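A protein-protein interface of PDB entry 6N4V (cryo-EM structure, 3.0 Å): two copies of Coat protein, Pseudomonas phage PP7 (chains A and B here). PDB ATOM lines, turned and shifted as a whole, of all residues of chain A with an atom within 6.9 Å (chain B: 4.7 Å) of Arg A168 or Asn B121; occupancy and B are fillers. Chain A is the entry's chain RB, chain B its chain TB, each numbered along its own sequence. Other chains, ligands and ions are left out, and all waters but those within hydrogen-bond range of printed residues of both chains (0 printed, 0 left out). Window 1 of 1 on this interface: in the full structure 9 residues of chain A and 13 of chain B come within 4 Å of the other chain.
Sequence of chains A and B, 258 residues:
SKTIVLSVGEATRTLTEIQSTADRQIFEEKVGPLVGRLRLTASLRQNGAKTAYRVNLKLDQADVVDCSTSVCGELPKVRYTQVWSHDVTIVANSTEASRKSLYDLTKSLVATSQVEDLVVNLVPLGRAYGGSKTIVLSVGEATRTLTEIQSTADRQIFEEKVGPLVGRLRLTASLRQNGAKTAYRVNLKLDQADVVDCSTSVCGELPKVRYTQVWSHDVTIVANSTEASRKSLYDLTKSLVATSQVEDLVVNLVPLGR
No position is printed for both chains. Of the 6 pairs that touch across the chains among the printed residues, none has its exchanged pair printed and touching as well.
O of Lys A161 sits at hydrogen-bond distance from NH2 of Arg A168, at 2.4 Å. O of Pro A164 is in hydrogen-bond range of NE of Arg A168 (3.0 Å). The backbone carbonyl oxygen (O) of Asp B117 lies within hydrogen-bond range of the backbone NH (N) of Leu B122. The backbone carbonyl oxygen (O) of Asp B117 sits at hydrogen-bond distance from the backbone NH (N) of Val B123 (3.0 Å). The guanidinium group (NE) of Arg B230 lies within hydrogen-bond range of the backbone carbonyl oxygen (O) of Val B120 (2.8 Å).
Of the 18 printed residues of chain A, 3 touch a printed residue of chain B. Of the 9 printed residues of chain B, 4 touch a printed residue of chain A. Hydrophobic or aromatic side chains of chain B that line the printed part of chain A: Leu B122 and Val B123. Among the printed residues, 6 pairs touch across the chains. Among the printed residues, no Asp or Glu carboxylate lies within 4 Å of a Lys or Arg side-chain nitrogen of the other chain.
Among the printed residues, pairs that only touch across the chains: Lys A161 with Asn B121 (3.4 Å), Leu A165 with Arg B230 (3.4 Å), Arg A168 with Asn B121 (3.6 Å), Leu A165 with Leu B122 (3.7 Å) and Lys A161 with Val B123 (3.8 Å).
Of the printed residues of chain B, Lys A161 touches Asn B121 (3.4 Å), Leu B122 (3.4 Å) and Val B123 (3.8 Å). Val A162 touches none of the printed residues of chain B. Of the printed residues of chain B, Leu A165 touches Leu B122 (3.7 Å) and Arg B230 (3.4 Å). Arg A168 touches just one residue of chain B: Asn B121. Asn B121 touches two residues of chain A. Of the printed residues of chain A, Val B123 touches Lys A161. Printed residues of chain A within 4 Å of Arg B230: Leu A165 (3.4 Å). The nearest residue of chain A that does not touch Asn B121 is Leu A165 (4.9 Å).
The backbone carbonyl oxygen of Leu B122 lies within hydrogen-bond range of the side-chain amino group of Lys A161, at 3.4 Å.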
ATOM      1  N   ARG A 144     -19.905 -20.404 -20.836  1.00  0.00           N
ATOM      2  CA  ARG A 144     -20.004 -19.549 -19.657  1.00  0.00           C
ATOM      3  C   ARG A 144     -18.894 -19.951 -18.693  1.00  0.00           C
ATOM      4  O   ARG A 144     -18.976 -20.986 -18.028  1.00  0.00           O
ATOM      5  CB  ARG A 144     -21.386 -19.665 -19.026  1.00  0.00           C
ATOM      6  CG  ARG A 144     -22.512 -19.466 -20.021  1.00  0.00           C
ATOM      7  CD  ARG A 144     -23.820 -19.134 -19.339  1.00  0.00           C
ATOM      8  NE  ARG A 144     -23.670 -18.065 -18.362  1.00  0.00           N
ATOM      9  CZ  ARG A 144     -24.673 -17.566 -17.651  1.00  0.00           C
ATOM     10  NH1 ARG A 144     -25.899 -18.038 -17.813  1.00  0.00           N
ATOM     11  NH2 ARG A 144     -24.453 -16.595 -16.779  1.00  0.00           N
ATOM     12  N   GLU A 159     -17.499 -18.224  -9.690  1.00  0.00           N
ATOM     13  CA  GLU A 159     -18.425 -17.156 -10.032  1.00  0.00           C
ATOM     14  C   GLU A 159     -18.108 -16.660 -11.434  1.00  0.00           C
ATOM     15  O   GLU A 159     -16.940 -16.563 -11.807  1.00  0.00           O
ATOM     16  CB  GLU A 159     -18.332 -16.005  -9.022  1.00  0.00           C
ATOM     17  CG  GLU A 159     -19.368 -14.917  -9.190  1.00  0.00           C
ATOM     18  CD  GLU A 159     -19.854 -14.373  -7.865  1.00  0.00           C
ATOM     19  OE1 GLU A 159     -19.585 -15.007  -6.825  1.00  0.00           O
ATOM     20  OE2 GLU A 159     -20.501 -13.307  -7.861  1.00  0.00           O
ATOM     21  N   GLU A 160     -19.149 -16.367 -12.206  1.00  0.00           N
ATOM     22  CA  GLU A 160     -18.961 -15.727 -13.497  1.00  0.00           C
ATOM     23  C   GLU A 160     -18.632 -14.255 -13.295  1.00  0.00           C
ATOM     24  O   GLU A 160     -18.916 -13.675 -12.245  1.00  0.00           O
ATOM     25  CB  GLU A 160     -20.206 -15.874 -14.366  1.00  0.00           C
ATOM     26  CG  GLU A 160     -19.897 -16.063 -15.834  1.00  0.00           C
ATOM     27  CD  GLU A 160     -21.112 -15.887 -16.709  1.00  0.00           C
ATOM     28  OE1 GLU A 160     -22.210 -15.663 -16.161  1.00  0.00           O
ATOM     29  OE2 GLU A 160     -20.970 -15.966 -17.946  1.00  0.00           O
ATOM     30  N   LYS A 161     -18.026 -13.645 -14.312  1.00  0.00           N
ATOM     31  CA  LYS A 161     -17.492 -12.300 -14.166  1.00  0.00           C
ATOM     32  C   LYS A 161     -18.082 -11.278 -15.126  1.00  0.00           C
ATOM     33  O   LYS A 161     -17.898 -10.077 -14.904  1.00  0.00           O
ATOM     34  CB  LYS A 161     -15.966 -12.320 -14.325  1.00  0.00           C
ATOM     35  CG  LYS A 161     -15.244 -12.931 -13.136  1.00  0.00           C
ATOM     36  CD  LYS A 161     -15.738 -12.339 -11.829  1.00  0.00           C
ATOM     37  CE  LYS A 161     -15.047 -12.964 -10.637  1.00  0.00           C
ATOM     38  NZ  LYS A 161     -15.572 -12.398  -9.370  1.00  0.00           N
ATOM     39  N   VAL A 162     -18.776 -11.700 -16.168  1.00  0.00           N
ATOM     40  CA  VAL A 162     -19.382 -10.746 -17.088  1.00  0.00           C
ATOM     41  C   VAL A 162     -20.701 -10.249 -16.513  1.00  0.00           C
ATOM     42  O   VAL A 162     -21.295 -10.871 -15.625  1.00  0.00           O
ATOM     43  CB  VAL A 162     -19.569 -11.378 -18.480  1.00  0.00           C
ATOM     44  CG1 VAL A 162     -18.238 -11.875 -19.013  1.00  0.00           C
ATOM     45  CG2 VAL A 162     -20.578 -12.510 -18.420  1.00  0.00           C
ATOM     46  N   GLY A 163     -21.156  -9.101 -17.009  1.00  0.00           N
ATOM     47  CA  GLY A 163     -22.439  -8.559 -16.633  1.00  0.00           C
ATOM     48  C   GLY A 163     -22.392  -7.726 -15.368  1.00  0.00           C
ATOM     49  O   GLY A 163     -21.326  -7.292 -14.924  1.00  0.00           O
ATOM     50  N   PRO A 164     -23.556  -7.480 -14.769  1.00  0.00           N
ATOM     51  CA  PRO A 164     -23.608  -6.699 -13.528  1.00  0.00           C
ATOM     52  C   PRO A 164     -23.051  -7.479 -12.347  1.00  0.00           C
ATOM     53  O   PRO A 164     -22.794  -8.681 -12.413  1.00  0.00           O
ATOM     54  CB  PRO A 164     -25.102  -6.417 -13.344  1.00  0.00           C
ATOM     55  CG  PRO A 164     -25.718  -6.678 -14.678  1.00  0.00           C
ATOM     56  CD  PRO A 164     -24.901  -7.761 -15.291  1.00  0.00           C
ATOM     57  N   LEU A 165     -22.872  -6.765 -11.241  1.00  0.00           N
ATOM     58  CA  LEU A 165     -22.299  -7.348 -10.035  1.00  0.00           C
ATOM     59  C   LEU A 165     -23.340  -7.873  -9.062  1.00  0.00           C
ATOM     60  O   LEU A 165     -22.975  -8.542  -8.092  1.00  0.00           O
ATOM     61  CB  LEU A 165     -21.429  -6.319  -9.307  1.00  0.00           C
ATOM     62  CG  LEU A 165     -20.462  -5.476 -10.134  1.00  0.00           C
ATOM     63  CD1 LEU A 165     -19.797  -4.444  -9.249  1.00  0.00           C
ATOM     64  CD2 LEU A 165     -19.424  -6.347 -10.803  1.00  0.00           C
ATOM     65  N   VAL A 166     -24.623  -7.588  -9.288  1.00  0.00           N
ATOM     66  CA  VAL A 166     -25.632  -7.972  -8.307  1.00  0.00           C
ATOM     67  C   VAL A 166     -26.053  -9.433  -8.461  1.00  0.00           C
ATOM     68  O   VAL A 166     -26.227 -10.135  -7.459  1.00  0.00           O
ATOM     69  CB  VAL A 166     -26.833  -7.010  -8.371  1.00  0.00           C
ATOM     70  CG1 VAL A 166     -26.450  -5.675  -7.780  1.00  0.00           C
ATOM     71  CG2 VAL A 166     -27.280  -6.793  -9.807  1.00  0.00           C
ATOM     72  N   GLY A 167     -26.220  -9.920  -9.686  1.00  0.00           N
ATOM     73  CA  GLY A 167     -26.589 -11.305  -9.889  1.00  0.00           C
ATOM     74  C   GLY A 167     -25.664 -12.015 -10.851  1.00  0.00           C
ATOM     75  O   GLY A 167     -25.623 -11.686 -12.039  1.00  0.00           O
ATOM     76  N   ARG A 168     -24.919 -12.995 -10.351  1.00  0.00           N
ATOM     77  CA  ARG A 168     -23.995 -13.756 -11.174  1.00  0.00           C
ATOM     78  C   ARG A 168     -24.116 -15.230 -10.825  1.00  0.00           C
ATOM     79  O   ARG A 168     -24.728 -15.602  -9.821  1.00  0.00           O
ATOM     80  CB  ARG A 168     -22.553 -13.272 -10.988  1.00  0.00           C
ATOM     81  CG  ARG A 168     -22.198 -12.064 -11.831  1.00  0.00           C
ATOM     82  CD  ARG A 168     -21.035 -11.300 -11.233  1.00  0.00           C
ATOM     83  NE  ARG A 168     -20.402 -10.420 -12.209  1.00  0.00           N
ATOM     84  CZ  ARG A 168     -19.279  -9.746 -11.987  1.00  0.00           C
ATOM     85  NH1 ARG A 168     -18.660  -9.854 -10.820  1.00  0.00           N
ATOM     86  NH2 ARG A 168     -18.774  -8.966 -12.930  1.00  0.00           N
ATOM     87  N   LEU A 169     -23.534 -16.069 -11.678  1.00  0.00           N
ATOM     88  CA  LEU A 169     -23.533 -17.503 -11.439  1.00  0.00           C
ATOM     89  C   LEU A 169     -22.660 -17.850 -10.241  1.00  0.00           C
ATOM     90  O   LEU A 169     -21.766 -17.098  -9.857  1.00  0.00           O
ATOM     91  CB  LEU A 169     -23.041 -18.251 -12.674  1.00  0.00           C
ATOM     92  CG  LEU A 169     -24.116 -18.809 -13.602  1.00  0.00           C
ATOM     93  CD1 LEU A 169     -23.484 -19.472 -14.800  1.00  0.00           C
ATOM     94  CD2 LEU A 169     -24.973 -19.795 -12.853  1.00  0.00           C
ATOM     95  N   ARG A 170     -22.937 -19.002  -9.643  1.00  0.00           N
ATOM     96  CA  ARG A 170     -22.210 -19.451  -8.470  1.00  0.00           C
ATOM     97  C   ARG A 170     -21.970 -20.946  -8.580  1.00  0.00           C
ATOM     98  O   ARG A 170     -22.719 -21.668  -9.237  1.00  0.00           O
ATOM     99  CB  ARG A 170     -22.973 -19.135  -7.181  1.00  0.00           C
ATOM    100  CG  ARG A 170     -22.670 -17.776  -6.597  1.00  0.00           C
ATOM    101  CD  ARG A 170     -21.334 -17.781  -5.899  1.00  0.00           C
ATOM    102  NE  ARG A 170     -20.965 -16.456  -5.414  1.00  0.00           N
ATOM    103  CZ  ARG A 170     -20.951 -16.107  -4.133  1.00  0.00           C
ATOM    104  NH1 ARG A 170     -21.287 -16.988  -3.202  1.00  0.00           N
ATOM    105  NH2 ARG A 170     -20.601 -14.879  -3.783  1.00  0.00           N
ATOM    106  N   ASP A 191     -26.034 -21.677  -8.007  1.00  0.00           N
ATOM    107  CA  ASP A 191     -27.053 -20.650  -7.851  1.00  0.00           C
ATOM    108  C   ASP A 191     -27.189 -19.860  -9.142  1.00  0.00           C
ATOM    109  O   ASP A 191     -26.191 -19.484  -9.759  1.00  0.00           O
ATOM    110  CB  ASP A 191     -26.693 -19.698  -6.713  1.00  0.00           C
ATOM    111  CG  ASP A 191     -26.632 -20.387  -5.373  1.00  0.00           C
ATOM    112  OD1 ASP A 191     -27.314 -21.410  -5.204  1.00  0.00           O
ATOM    113  OD2 ASP A 191     -25.901 -19.903  -4.486  1.00  0.00           O
ATOM    114  N   GLN A 192     -28.430 -19.599  -9.541  1.00  0.00           N
ATOM    115  CA  GLN A 192     -28.698 -18.775 -10.711  1.00  0.00           C
ATOM    116  C   GLN A 192     -29.778 -17.773 -10.350  1.00  0.00           C
ATOM    117  O   GLN A 192     -30.928 -18.155 -10.117  1.00  0.00           O
ATOM    118  CB  GLN A 192     -29.130 -19.619 -11.909  1.00  0.00           C
ATOM    119  CG  GLN A 192     -28.976 -18.908 -13.235  1.00  0.00           C
ATOM    120  CD  GLN A 192     -29.966 -19.384 -14.268  1.00  0.00           C
ATOM    121  OE1 GLN A 192     -31.132 -19.616 -13.961  1.00  0.00           O
ATOM    122  NE2 GLN A 192     -29.506 -19.534 -15.502  1.00  0.00           N
ATOM    123  N   ALA A 193     -29.409 -16.501 -10.300  1.00  0.00           N
ATOM    124  CA  ALA A 193     -30.331 -15.424  -9.982  1.00  0.00           C
ATOM    125  C   ALA A 193     -30.749 -14.716 -11.261  1.00  0.00           C
ATOM    126  O   ALA A 193     -29.938 -14.537 -12.175  1.00  0.00           O
ATOM    127  CB  ALA A 193     -29.697 -14.425  -9.014  1.00  0.00           C
ATOM    128  N   VAL A 195     -31.691 -11.420 -13.000  1.00  0.00           N
ATOM    129  CA  VAL A 195     -31.515  -9.982 -12.847  1.00  0.00           C
ATOM    130  C   VAL A 195     -32.200  -9.276 -14.012  1.00  0.00           C
ATOM    131  O   VAL A 195     -32.124  -9.724 -15.164  1.00  0.00           O
ATOM    132  CB  VAL A 195     -30.015  -9.625 -12.731  1.00  0.00           C
ATOM    133  CG1 VAL A 195     -29.199 -10.195 -13.890  1.00  0.00           C
ATOM    134  CG2 VAL A 195     -29.797  -8.126 -12.598  1.00  0.00           C
ATOM    135  N   VAL A 209     -32.131  -8.245  -8.493  1.00  0.00           N
ATOM    136  CA  VAL A 209     -32.451  -9.657  -8.664  1.00  0.00           C
ATOM    137  C   VAL A 209     -33.911  -9.894  -8.314  1.00  0.00           C
ATOM    138  O   VAL A 209     -34.449  -9.293  -7.376  1.00  0.00           O
ATOM    139  CB  VAL A 209     -31.524 -10.545  -7.813  1.00  0.00           C
ATOM    140  CG1 VAL A 209     -30.165 -10.659  -8.468  1.00  0.00           C
ATOM    141  CG2 VAL A 209     -31.380  -9.986  -6.410  1.00  0.00           C
ATOM    142  N   GLU B 116      -7.081  -3.517 -13.536  1.00  0.00           N
ATOM    143  CA  GLU B 116      -8.244  -3.041 -14.277  1.00  0.00           C
ATOM    144  C   GLU B 116      -9.433  -3.975 -14.102  1.00  0.00           C
ATOM    145  O   GLU B 116     -10.545  -3.523 -13.817  1.00  0.00           O
ATOM    146  CB  GLU B 116      -7.899  -2.894 -15.757  1.00  0.00           C
ATOM    147  CG  GLU B 116      -9.101  -2.620 -16.641  1.00  0.00           C
ATOM    148  CD  GLU B 116      -8.724  -2.391 -18.085  1.00  0.00           C
ATOM    149  OE1 GLU B 116      -7.526  -2.511 -18.415  1.00  0.00           O
ATOM    150  OE2 GLU B 116      -9.624  -2.089 -18.893  1.00  0.00           O
ATOM    151  N   ASP B 117      -9.212  -5.284 -14.225  1.00  0.00           N
ATOM    152  CA  ASP B 117     -10.291  -6.239 -14.013  1.00  0.00           C
ATOM    153  C   ASP B 117     -10.651  -6.395 -12.543  1.00  0.00           C
ATOM    154  O   ASP B 117     -11.715  -6.937 -12.235  1.00  0.00           O
ATOM    155  CB  ASP B 117      -9.913  -7.596 -14.592  1.00  0.00           C
ATOM    156  CG  ASP B 117      -9.436  -7.501 -16.018  1.00  0.00           C
ATOM    157  OD1 ASP B 117      -9.718  -6.479 -16.672  1.00  0.00           O
ATOM    158  OD2 ASP B 117      -8.778  -8.451 -16.490  1.00  0.00           O
ATOM    159  N   VAL B 119     -11.134  -3.839 -10.403  1.00  0.00           N
ATOM    160  CA  VAL B 119     -12.057  -2.786  -9.997  1.00  0.00           C
ATOM    161  C   VAL B 119     -13.254  -2.736 -10.937  1.00  0.00           C
ATOM    162  O   VAL B 119     -14.327  -2.260 -10.560  1.00  0.00           O
ATOM    163  CB  VAL B 119     -11.349  -1.423  -9.920  1.00  0.00           C
ATOM    164  CG1 VAL B 119     -10.339  -1.428  -8.794  1.00  0.00           C
ATOM    165  CG2 VAL B 119     -10.668  -1.096 -11.230  1.00  0.00           C
ATOM    166  N   VAL B 120     -13.096  -3.234 -12.161  1.00  0.00           N
ATOM    167  CA  VAL B 120     -14.222  -3.232 -13.087  1.00  0.00           C
ATOM    168  C   VAL B 120     -15.054  -4.498 -12.931  1.00  0.00           C
ATOM    169  O   VAL B 120     -16.255  -4.436 -12.654  1.00  0.00           O
ATOM    170  CB  VAL B 120     -13.733  -3.049 -14.534  1.00  0.00           C
ATOM    171  CG1 VAL B 120     -14.876  -3.245 -15.501  1.00  0.00           C
ATOM    172  CG2 VAL B 120     -13.134  -1.676 -14.712  1.00  0.00           C
ATOM    173  N   ASN B 121     -14.432  -5.665 -13.094  1.00  0.00           N
ATOM    174  CA  ASN B 121     -15.150  -6.932 -13.099  1.00  0.00           C
ATOM    175  C   ASN B 121     -14.902  -7.765 -11.850  1.00  0.00           C
ATOM    176  O   ASN B 121     -15.303  -8.932 -11.819  1.00  0.00           O
ATOM    177  CB  ASN B 121     -14.778  -7.740 -14.340  1.00  0.00           C
ATOM    178  CG  ASN B 121     -15.308  -7.128 -15.612  1.00  0.00           C
ATOM    179  OD1 ASN B 121     -16.450  -6.678 -15.668  1.00  0.00           O
ATOM    180  ND2 ASN B 121     -14.477  -7.104 -16.646  1.00  0.00           N
ATOM    181  N   LEU B 122     -14.222  -7.205 -10.847  1.00  0.00           N
ATOM    182  CA  LEU B 122     -14.011  -7.791  -9.518  1.00  0.00           C
ATOM    183  C   LEU B 122     -13.230  -9.105  -9.556  1.00  0.00           C
ATOM    184  O   LEU B 122     -13.331  -9.915  -8.631  1.00  0.00           O
ATOM    185  CB  LEU B 122     -15.336  -7.983  -8.765  1.00  0.00           C
ATOM    186  CG  LEU B 122     -15.890  -6.836  -7.910  1.00  0.00           C
ATOM    187  CD1 LEU B 122     -14.912  -6.427  -6.841  1.00  0.00           C
ATOM    188  CD2 LEU B 122     -16.280  -5.632  -8.742  1.00  0.00           C
ATOM    189  N   VAL B 123     -12.441  -9.325 -10.599  1.00  0.00           N
ATOM    190  CA  VAL B 123     -11.615 -10.530 -10.706  1.00  0.00           C
ATOM    191  C   VAL B 123     -10.404 -10.376  -9.791  1.00  0.00           C
ATOM    192  O   VAL B 123      -9.771  -9.312  -9.801  1.00  0.00           O
ATOM    193  CB  VAL B 123     -11.183 -10.748 -12.152  1.00  0.00           C
ATOM    194  CG1 VAL B 123     -10.622 -12.138 -12.341  1.00  0.00           C
ATOM    195  CG2 VAL B 123     -12.345 -10.519 -13.089  1.00  0.00           C
ATOM    196  N   GLU B 227     -21.203  -0.495 -15.650  1.00  0.00           N
ATOM    197  CA  GLU B 227     -19.852  -0.914 -16.009  1.00  0.00           C
ATOM    198  C   GLU B 227     -19.008   0.265 -16.465  1.00  0.00           C
ATOM    199  O   GLU B 227     -17.833   0.367 -16.097  1.00  0.00           O
ATOM    200  CB  GLU B 227     -19.895  -1.988 -17.094  1.00  0.00           C
ATOM    201  CG  GLU B 227     -18.522  -2.467 -17.540  1.00  0.00           C
ATOM    202  CD  GLU B 227     -18.584  -3.731 -18.366  1.00  0.00           C
ATOM    203  OE1 GLU B 227     -19.490  -4.555 -18.128  1.00  0.00           O
ATOM    204  OE2 GLU B 227     -17.723  -3.901 -19.254  1.00  0.00           O
ATOM    205  N   ARG B 230     -17.605   2.236 -13.436  1.00  0.00           N
ATOM    206  CA  ARG B 230     -16.365   1.741 -12.850  1.00  0.00           C
ATOM    207  C   ARG B 230     -15.208   1.833 -13.834  1.00  0.00           C
ATOM    208  O   ARG B 230     -14.052   1.949 -13.418  1.00  0.00           O
ATOM    209  CB  ARG B 230     -16.536   0.299 -12.385  1.00  0.00           C
ATOM    210  CG  ARG B 230     -17.770   0.056 -11.544  1.00  0.00           C
ATOM    211  CD  ARG B 230     -17.905  -1.411 -11.187  1.00  0.00           C
ATOM    212  NE  ARG B 230     -17.978  -2.261 -12.369  1.00  0.00           N
ATOM    213  CZ  ARG B 230     -19.092  -2.836 -12.804  1.00  0.00           C
ATOM    214  NH1 ARG B 230     -20.228  -2.649 -12.154  1.00  0.00           N
ATOM    215  NH2 ARG B 230     -19.072  -3.596 -13.888  1.00  0.00           N
